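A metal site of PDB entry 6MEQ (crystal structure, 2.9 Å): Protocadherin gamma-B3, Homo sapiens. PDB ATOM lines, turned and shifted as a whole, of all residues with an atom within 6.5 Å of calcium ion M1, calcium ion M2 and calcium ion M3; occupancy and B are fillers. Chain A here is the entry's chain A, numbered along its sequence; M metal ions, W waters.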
ATOM      1  N   GLU A 223      11.671 -11.362 -10.938  1.00  0.00           N
ATOM      2  CA  GLU A 223      11.987 -10.765  -9.642  1.00  0.00           C
ATOM      3  C   GLU A 223      12.549  -9.367  -9.808  1.00  0.00           C
ATOM      4  O   GLU A 223      12.025  -8.398  -9.240  1.00  0.00           O
ATOM      5  CB  GLU A 223      12.981 -11.658  -8.888  1.00  0.00           C
ATOM      6  CG  GLU A 223      13.166 -11.282  -7.428  1.00  0.00           C
ATOM      7  CD  GLU A 223      14.351 -11.977  -6.796  1.00  0.00           C
ATOM      8  OE1 GLU A 223      15.361 -11.288  -6.514  1.00  0.00           O
ATOM      9  OE2 GLU A 223      14.279 -13.202  -6.579  1.00  0.00           O
ATOM     10  N   ASN A 224      13.622  -9.224 -10.582  1.00  0.00           N
ATOM     11  CA  ASN A 224      14.263  -7.929 -10.800  1.00  0.00           C
ATOM     12  C   ASN A 224      13.651  -7.217 -12.005  1.00  0.00           C
ATOM     13  O   ASN A 224      14.320  -6.876 -12.983  1.00  0.00           O
ATOM     14  CB  ASN A 224      15.773  -8.102 -10.950  1.00  0.00           C
ATOM     15  CG  ASN A 224      16.426  -8.656  -9.705  1.00  0.00           C
ATOM     16  OD1 ASN A 224      15.967  -8.420  -8.587  1.00  0.00           O
ATOM     17  ND2 ASN A 224      17.508  -9.408  -9.888  1.00  0.00           N
ATOM     18  N   LEU A 277      10.664  -5.051  -6.983  1.00  0.00           N
ATOM     19  CA  LEU A 277      10.127  -6.327  -6.554  1.00  0.00           C
ATOM     20  C   LEU A 277      11.240  -7.191  -5.957  1.00  0.00           C
ATOM     21  O   LEU A 277      12.400  -7.083  -6.336  1.00  0.00           O
ATOM     22  CB  LEU A 277       9.476  -7.058  -7.733  1.00  0.00           C
ATOM     23  CG  LEU A 277       8.356  -6.327  -8.462  1.00  0.00           C
ATOM     24  CD1 LEU A 277       7.803  -7.176  -9.599  1.00  0.00           C
ATOM     25  CD2 LEU A 277       7.249  -5.939  -7.492  1.00  0.00           C
ATOM     26  N   ASP A 278      10.856  -8.046  -5.012  1.00  0.00           N
ATOM     27  CA  ASP A 278      11.815  -8.916  -4.340  1.00  0.00           C
ATOM     28  C   ASP A 278      11.121 -10.205  -3.943  1.00  0.00           C
ATOM     29  O   ASP A 278      10.140 -10.176  -3.183  1.00  0.00           O
ATOM     30  CB  ASP A 278      12.408  -8.219  -3.104  1.00  0.00           C
ATOM     31  CG  ASP A 278      13.602  -8.968  -2.533  1.00  0.00           C
ATOM     32  OD1 ASP A 278      14.040  -9.953  -3.155  1.00  0.00           O
ATOM     33  OD2 ASP A 278      14.087  -8.571  -1.456  1.00  0.00           O
ATOM     34  N   PHE A 279      11.618 -11.330  -4.465  1.00  0.00           N
ATOM     35  CA  PHE A 279      11.014 -12.622  -4.138  1.00  0.00           C
ATOM     36  C   PHE A 279      11.291 -13.028  -2.703  1.00  0.00           C
ATOM     37  O   PHE A 279      10.449 -13.686  -2.072  1.00  0.00           O
ATOM     38  CB  PHE A 279      11.532 -13.684  -5.110  1.00  0.00           C
ATOM     39  CG  PHE A 279      10.964 -15.058  -4.877  1.00  0.00           C
ATOM     40  CD1 PHE A 279       9.767 -15.433  -5.454  1.00  0.00           C
ATOM     41  CD2 PHE A 279      11.636 -15.975  -4.085  1.00  0.00           C
ATOM     42  CE1 PHE A 279       9.239 -16.696  -5.245  1.00  0.00           C
ATOM     43  CE2 PHE A 279      11.113 -17.238  -3.867  1.00  0.00           C
ATOM     44  CZ  PHE A 279       9.918 -17.599  -4.443  1.00  0.00           C
ATOM     45  N   GLU A 280      12.460 -12.662  -2.169  1.00  0.00           N
ATOM     46  CA  GLU A 280      12.801 -13.027  -0.794  1.00  0.00           C
ATOM     47  C   GLU A 280      11.941 -12.316   0.235  1.00  0.00           C
ATOM     48  O   GLU A 280      11.866 -12.763   1.378  1.00  0.00           O
ATOM     49  CB  GLU A 280      14.279 -12.741  -0.531  1.00  0.00           C
ATOM     50  CG  GLU A 280      15.240 -13.768  -1.113  1.00  0.00           C
ATOM     51  CD  GLU A 280      15.303 -13.729  -2.623  1.00  0.00           C
ATOM     52  OE1 GLU A 280      15.009 -12.660  -3.210  1.00  0.00           O
ATOM     53  OE2 GLU A 280      15.643 -14.764  -3.236  1.00  0.00           O
ATOM     54  N   SER A 308       8.486 -14.670  -9.728  1.00  0.00           N
ATOM     55  CA  SER A 308       9.403 -15.797  -9.828  1.00  0.00           C
ATOM     56  C   SER A 308      10.755 -15.430  -9.233  1.00  0.00           C
ATOM     57  O   SER A 308      11.174 -14.276  -9.277  1.00  0.00           O
ATOM     58  CB  SER A 308       9.565 -16.240 -11.282  1.00  0.00           C
ATOM     59  OG  SER A 308      10.061 -15.184 -12.083  1.00  0.00           O
ATOM     60  N   ASP A 309      11.440 -16.430  -8.699  1.00  0.00           N
ATOM     61  CA  ASP A 309      12.725 -16.209  -8.054  1.00  0.00           C
ATOM     62  C   ASP A 309      13.844 -16.104  -9.078  1.00  0.00           C
ATOM     63  O   ASP A 309      13.905 -16.892 -10.031  1.00  0.00           O
ATOM     64  CB  ASP A 309      13.034 -17.342  -7.066  1.00  0.00           C
ATOM     65  CG  ASP A 309      14.393 -17.192  -6.419  1.00  0.00           C
ATOM     66  OD1 ASP A 309      14.586 -16.237  -5.646  1.00  0.00           O
ATOM     67  OD2 ASP A 309      15.270 -18.049  -6.674  1.00  0.00           O
ATOM     68  N   GLU A 310      14.726 -15.128  -8.881  1.00  0.00           N
ATOM     69  CA  GLU A 310      15.897 -14.947  -9.714  1.00  0.00           C
ATOM     70  C   GLU A 310      17.157 -15.122  -8.875  1.00  0.00           C
ATOM     71  O   GLU A 310      17.171 -14.819  -7.684  1.00  0.00           O
ATOM     72  CB  GLU A 310      15.914 -13.552 -10.378  1.00  0.00           C
ATOM     73  CG  GLU A 310      14.867 -13.366 -11.461  1.00  0.00           C
ATOM     74  CD  GLU A 310      15.184 -14.148 -12.735  1.00  0.00           C
ATOM     75  OE1 GLU A 310      16.346 -14.567 -12.893  1.00  0.00           O
ATOM     76  OE2 GLU A 310      14.275 -14.324 -13.569  1.00  0.00           O
ATOM     77  N   ASN A 311      18.205 -15.641  -9.511  1.00  0.00           N
ATOM     78  CA  ASN A 311      19.482 -15.885  -8.835  1.00  0.00           C
ATOM     79  C   ASN A 311      20.260 -14.570  -8.781  1.00  0.00           C
ATOM     80  O   ASN A 311      21.160 -14.304  -9.582  1.00  0.00           O
ATOM     81  CB  ASN A 311      20.266 -16.981  -9.540  1.00  0.00           C
ATOM     82  CG  ASN A 311      21.567 -17.321  -8.832  1.00  0.00           C
ATOM     83  OD1 ASN A 311      21.703 -17.087  -7.633  1.00  0.00           O
ATOM     84  ND2 ASN A 311      22.513 -17.867  -9.573  1.00  0.00           N
ATOM     85  N   ASP A 312      19.906 -13.737  -7.801  1.00  0.00           N
ATOM     86  CA  ASP A 312      20.567 -12.457  -7.602  1.00  0.00           C
ATOM     87  C   ASP A 312      21.245 -12.367  -6.233  1.00  0.00           C
ATOM     88  O   ASP A 312      21.661 -11.270  -5.839  1.00  0.00           O
ATOM     89  CB  ASP A 312      19.568 -11.305  -7.758  1.00  0.00           C
ATOM     90  CG  ASP A 312      18.466 -11.342  -6.713  1.00  0.00           C
ATOM     91  OD1 ASP A 312      18.079 -12.440  -6.287  1.00  0.00           O
ATOM     92  OD2 ASP A 312      17.995 -10.246  -6.319  1.00  0.00           O
ATOM     93  N   ASN A 313      21.381 -13.472  -5.524  1.00  0.00           N
ATOM     94  CA  ASN A 313      22.056 -13.519  -4.230  1.00  0.00           C
ATOM     95  C   ASN A 313      23.237 -14.465  -4.311  1.00  0.00           C
ATOM     96  O   ASN A 313      23.098 -15.610  -4.770  1.00  0.00           O
ATOM     97  CB  ASN A 313      21.095 -13.957  -3.123  1.00  0.00           C
ATOM     98  CG  ASN A 313      20.112 -12.872  -2.734  1.00  0.00           C
ATOM     99  OD1 ASN A 313      20.373 -12.073  -1.845  1.00  0.00           O
ATOM    100  ND2 ASN A 313      18.967 -12.846  -3.414  1.00  0.00           N
ATOM    101  N   ALA A 314      24.401 -13.993  -3.868  1.00  0.00           N
ATOM    102  CA  ALA A 314      25.623 -14.790  -3.873  1.00  0.00           C
ATOM    103  C   ALA A 314      25.716 -15.631  -2.600  1.00  0.00           C
ATOM    104  O   ALA A 314      25.227 -15.233  -1.539  1.00  0.00           O
ATOM    105  CB  ALA A 314      26.845 -13.895  -3.978  1.00  0.00           C
ATOM    106  N   PRO A 315      26.326 -16.810  -2.687  1.00  0.00           N
ATOM    107  CA  PRO A 315      26.486 -17.645  -1.481  1.00  0.00           C
ATOM    108  C   PRO A 315      27.364 -16.960  -0.455  1.00  0.00           C
ATOM    109  O   PRO A 315      28.352 -16.300  -0.773  1.00  0.00           O
ATOM    110  CB  PRO A 315      27.143 -18.920  -2.018  1.00  0.00           C
ATOM    111  CG  PRO A 315      26.817 -18.941  -3.486  1.00  0.00           C
ATOM    112  CD  PRO A 315      26.794 -17.502  -3.903  1.00  0.00           C
ATOM    113  N   ASP A 343      22.234 -19.517   1.246  1.00  0.00           N
ATOM    114  CA  ASP A 343      21.889 -18.630   0.142  1.00  0.00           C
ATOM    115  C   ASP A 343      20.438 -18.205   0.285  1.00  0.00           C
ATOM    116  O   ASP A 343      19.553 -19.028   0.564  1.00  0.00           O
ATOM    117  CB  ASP A 343      22.106 -19.326  -1.212  1.00  0.00           C
ATOM    118  CG  ASP A 343      22.156 -18.342  -2.367  1.00  0.00           C
ATOM    119  OD1 ASP A 343      23.191 -17.674  -2.548  1.00  0.00           O
ATOM    120  OD2 ASP A 343      21.142 -18.232  -3.098  1.00  0.00           O
ATOM    121  N   LEU A 344      20.185 -16.910   0.083  1.00  0.00           N
ATOM    122  CA  LEU A 344      18.847 -16.364   0.275  1.00  0.00           C
ATOM    123  C   LEU A 344      17.875 -16.825  -0.806  1.00  0.00           C
ATOM    124  O   LEU A 344      16.659 -16.782  -0.587  1.00  0.00           O
ATOM    125  CB  LEU A 344      18.897 -14.835   0.325  1.00  0.00           C
ATOM    126  CG  LEU A 344      19.730 -14.230   1.455  1.00  0.00           C
ATOM    127  CD1 LEU A 344      19.659 -12.714   1.425  1.00  0.00           C
ATOM    128  CD2 LEU A 344      19.279 -14.773   2.806  1.00  0.00           C
ATOM    129  N   ASP A 345      18.371 -17.246  -1.959  1.00  0.00           N
ATOM    130  CA  ASP A 345      17.501 -17.673  -3.041  1.00  0.00           C
ATOM    131  C   ASP A 345      16.901 -19.049  -2.728  1.00  0.00           C
ATOM    132  O   ASP A 345      17.304 -19.738  -1.793  1.00  0.00           O
ATOM    133  CB  ASP A 345      18.264 -17.715  -4.367  1.00  0.00           C
ATOM    134  CG  ASP A 345      18.923 -16.385  -4.690  1.00  0.00           C
ATOM    135  OD1 ASP A 345      18.302 -15.337  -4.444  1.00  0.00           O
ATOM    136  OD2 ASP A 345      20.066 -16.395  -5.192  1.00  0.00           O
ATOM    137  N   SER A 346      15.925 -19.449  -3.547  1.00  0.00           N
ATOM    138  CA  SER A 346      15.219 -20.707  -3.378  1.00  0.00           C
ATOM    139  C   SER A 346      15.502 -21.628  -4.551  1.00  0.00           C
ATOM    140  O   SER A 346      16.113 -21.244  -5.557  1.00  0.00           O
ATOM    141  CB  SER A 346      13.705 -20.462  -3.241  1.00  0.00           C
ATOM    142  OG  SER A 346      13.428 -19.623  -2.130  1.00  0.00           O
ATOM    143  N   PHE A 348      17.059 -24.458  -6.931  1.00  0.00           N
ATOM    144  CA  PHE A 348      18.449 -24.743  -7.268  1.00  0.00           C
ATOM    145  C   PHE A 348      19.334 -23.506  -7.136  1.00  0.00           C
ATOM    146  O   PHE A 348      20.561 -23.640  -7.074  1.00  0.00           O
ATOM    147  CB  PHE A 348      18.553 -25.304  -8.687  1.00  0.00           C
ATOM    148  CG  PHE A 348      18.204 -26.760  -8.786  1.00  0.00           C
ATOM    149  CD1 PHE A 348      19.165 -27.728  -8.571  1.00  0.00           C
ATOM    150  CD2 PHE A 348      16.916 -27.152  -9.102  1.00  0.00           C
ATOM    151  CE1 PHE A 348      18.850 -29.066  -8.665  1.00  0.00           C
ATOM    152  CE2 PHE A 348      16.594 -28.497  -9.193  1.00  0.00           C
ATOM    153  CZ  PHE A 348      17.566 -29.459  -8.972  1.00  0.00           C
ATOM    154  N   ASN A 349      18.738 -22.312  -7.081  1.00  0.00           N
ATOM    155  CA  ASN A 349      19.509 -21.092  -6.877  1.00  0.00           C
ATOM    156  C   ASN A 349      20.032 -20.971  -5.452  1.00  0.00           C
ATOM    157  O   ASN A 349      20.901 -20.118  -5.202  1.00  0.00           O
ATOM    158  CB  ASN A 349      18.663 -19.870  -7.219  1.00  0.00           C
ATOM    159  CG  ASN A 349      18.124 -19.912  -8.636  1.00  0.00           C
ATOM    160  OD1 ASN A 349      18.755 -20.469  -9.534  1.00  0.00           O
ATOM    161  ND2 ASN A 349      16.962 -19.305  -8.838  1.00  0.00           N
ATOM    162  N   GLY A 350      19.547 -21.794  -4.521  1.00  0.00           N
ATOM    163  CA  GLY A 350      20.018 -21.757  -3.156  1.00  0.00           C
ATOM    164  C   GLY A 350      20.959 -22.895  -2.817  1.00  0.00           C
ATOM    165  O   GLY A 350      21.664 -22.841  -1.794  1.00  0.00           O
ATOM    166  N   GLU A 351      20.981 -23.936  -3.644  1.00  0.00           N
ATOM    167  CA  GLU A 351      21.881 -25.055  -3.432  1.00  0.00           C
ATOM    168  C   GLU A 351      23.322 -24.599  -3.639  1.00  0.00           C
ATOM    169  O   GLU A 351      23.679 -24.089  -4.705  1.00  0.00           O
ATOM    170  CB  GLU A 351      21.539 -26.198  -4.396  1.00  0.00           C
ATOM    171  CG  GLU A 351      20.087 -26.643  -4.337  1.00  0.00           C
ATOM    172  CD  GLU A 351      19.736 -27.312  -3.018  1.00  0.00           C
ATOM    173  OE1 GLU A 351      20.642 -27.877  -2.370  1.00  0.00           O
ATOM    174  OE2 GLU A 351      18.549 -27.262  -2.638  1.00  0.00           O
ATOM    175  N   ASP A 396      26.702 -21.402  -6.198  1.00  0.00           N
ATOM    176  CA  ASP A 396      25.336 -21.903  -6.262  1.00  0.00           C
ATOM    177  C   ASP A 396      25.104 -22.612  -7.590  1.00  0.00           C
ATOM    178  O   ASP A 396      25.971 -22.672  -8.459  1.00  0.00           O
ATOM    179  CB  ASP A 396      24.342 -20.755  -6.062  1.00  0.00           C
ATOM    180  CG  ASP A 396      24.514 -19.635  -7.064  1.00  0.00           C
ATOM    181  OD1 ASP A 396      24.145 -19.823  -8.238  1.00  0.00           O
ATOM    182  OD2 ASP A 396      25.027 -18.561  -6.676  1.00  0.00           O
ATOM    183  N   LYS A 397      23.899 -23.170  -7.753  1.00  0.00           N
ATOM    184  CA  LYS A 397      23.516 -23.903  -8.950  1.00  0.00           C
ATOM    185  C   LYS A 397      22.490 -23.131  -9.770  1.00  0.00           C
ATOM    186  O   LYS A 397      21.534 -23.707 -10.313  1.00  0.00           O
ATOM    187  CB  LYS A 397      22.966 -25.287  -8.586  1.00  0.00           C
ATOM    188  CG  LYS A 397      23.921 -26.144  -7.778  1.00  0.00           C
ATOM    189  CD  LYS A 397      23.283 -27.466  -7.397  1.00  0.00           C
ATOM    190  CE  LYS A 397      24.220 -28.310  -6.540  1.00  0.00           C
ATOM    191  NZ  LYS A 397      25.466 -28.663  -7.260  1.00  0.00           N
ATOM    192  N   GLY A 398      22.677 -21.816  -9.883  1.00  0.00           N
ATOM    193  CA  GLY A 398      21.770 -20.968 -10.616  1.00  0.00           C
ATOM    194  C   GLY A 398      22.221 -20.719 -12.051  1.00  0.00           C
ATOM    195  O   GLY A 398      23.228 -21.246 -12.518  1.00  0.00           O
ATOM    196  N   LEU A 402      26.332 -17.663  -9.267  1.00  0.00           N
ATOM    197  CA  LEU A 402      27.145 -16.717  -8.526  1.00  0.00           C
ATOM    198  C   LEU A 402      28.081 -17.475  -7.586  1.00  0.00           C
ATOM    199  O   LEU A 402      27.889 -18.651  -7.296  1.00  0.00           O
ATOM    200  CB  LEU A 402      26.278 -15.733  -7.734  1.00  0.00           C
ATOM    201  CG  LEU A 402      25.591 -14.590  -8.488  1.00  0.00           C
ATOM    202  CD1 LEU A 402      24.415 -15.085  -9.321  1.00  0.00           C
ATOM    203  CD2 LEU A 402      25.137 -13.514  -7.509  1.00  0.00           C
HETATM  204 CA    CA M   1      16.152 -10.266  -4.455  1.00  0.00          CA
HETATM  205 CA    CA M   2      16.335 -14.025  -5.498  1.00  0.00          CA
HETATM  206 CA    CA M   3      22.310 -17.962  -5.260  1.00  0.00          CA
HETATM  207  O   HOH W   1      19.327  -9.213  -3.639  1.00  0.00           O
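Six residues have an atom within 4 Å of calcium ion M3: Asn 311, Asn 313, Asp 343, Asp 345, Asn 349 and Asp 396.
The nearest printed residue that does not touch calcium ion M3 is Ala 314 (4.7 Å).
Calcium ion M3 is bound by OD2 of Asp 343 (2.5 Å), O of Asn 313 (2.5 Å), O of Asn 349 (2.6 Å), OD1 of Asn 311 (2.6 Å), OD2 of Asp 345 (2.7 Å) and OD1 of Asp 343 (2.9 Å).
Calcium ion M3 has six donor atoms within binding distance.
Slightly farther from calcium ion M3 lies the side-chain carboxylate (OD2) of Asp 396 (3.1 Å).
Within 4 Å of calcium ion M1: Glu 223, Asp 278, Glu 280, Asp 312 and Asn 313.
The nearest printed residue that does not touch calcium ion M1 is Asn 224 (4.5 Å).
Calcium ion M1 is bound by the side-chain carboxylate (OE1) of Glu 223 (2.4 Å), the side-chain carboxylate (OD1) of Asp 278 (2.5 Å) and the side-chain carboxylate (OD2) of Asp 312 (2.6 Å).
Slightly farther from calcium ion M1 lies the side-chain carboxylate (OE1) of Glu 280 (2.9 Å).
OD1 of Asp 278 lies close to N of Glu 280, at 3.3 Å.
The backbone NH (N) of Leu 402 lies within hydrogen-bond range of the side-chain carboxylate (OD2) of Asp 396 (3.0 Å).
The side-chain carboxylate (OD2) of Asp 309 sits at hydrogen-bond distance from the side-chain amide nitrogen (ND2) of Asn 349 (3.0 Å).
The backbone NH of Gly 398 lies within hydrogen-bond range of the side-chain carboxylate of Asp 396 (3.0 Å).
N of Glu 223 sits close to O of Ser 308.
The side-chain carboxylate of Asp 309 is in hydrogen-bond range of the backbone NH of Ser 346 (3.5 Å).
ND2 of Asn 313 sits close to OD1 of Asp 312, 3.0 Å away.
The side-chain carboxylate of Asp 396 is in hydrogen-bond range of the side-chain amide nitrogen of Asn 311 (2.9 Å).
Calcium ion M2 is bound by the side-chain carboxylate of Glu 223 (2.5 Å), the backbone carbonyl oxygen of Glu 310 (2.5 Å), the side-chain carboxylate of Glu 280 (2.5 Å), the side-chain carboxylate of Asp 312 (2.5 Å), the side-chain carboxylate of Asp 345 (2.6 Å) and the side-chain carboxylate of Asp 309 (2.8 Å).
Calcium ion M2 has six donor atoms within binding distance.
Slightly farther from calcium ion M2 lies the side-chain carboxylate (OE1) of Glu 280 (3.0 Å).
Slightly farther from calcium ion M2 lies the side-chain carboxylate (OE1) of Glu 223 (3.1 Å).
Of the 26 residues printed, 7 come within 4 Å of calcium ion M2.
The nearest printed residue that does not touch calcium ion M2 is Asn 311 (4.7 Å).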
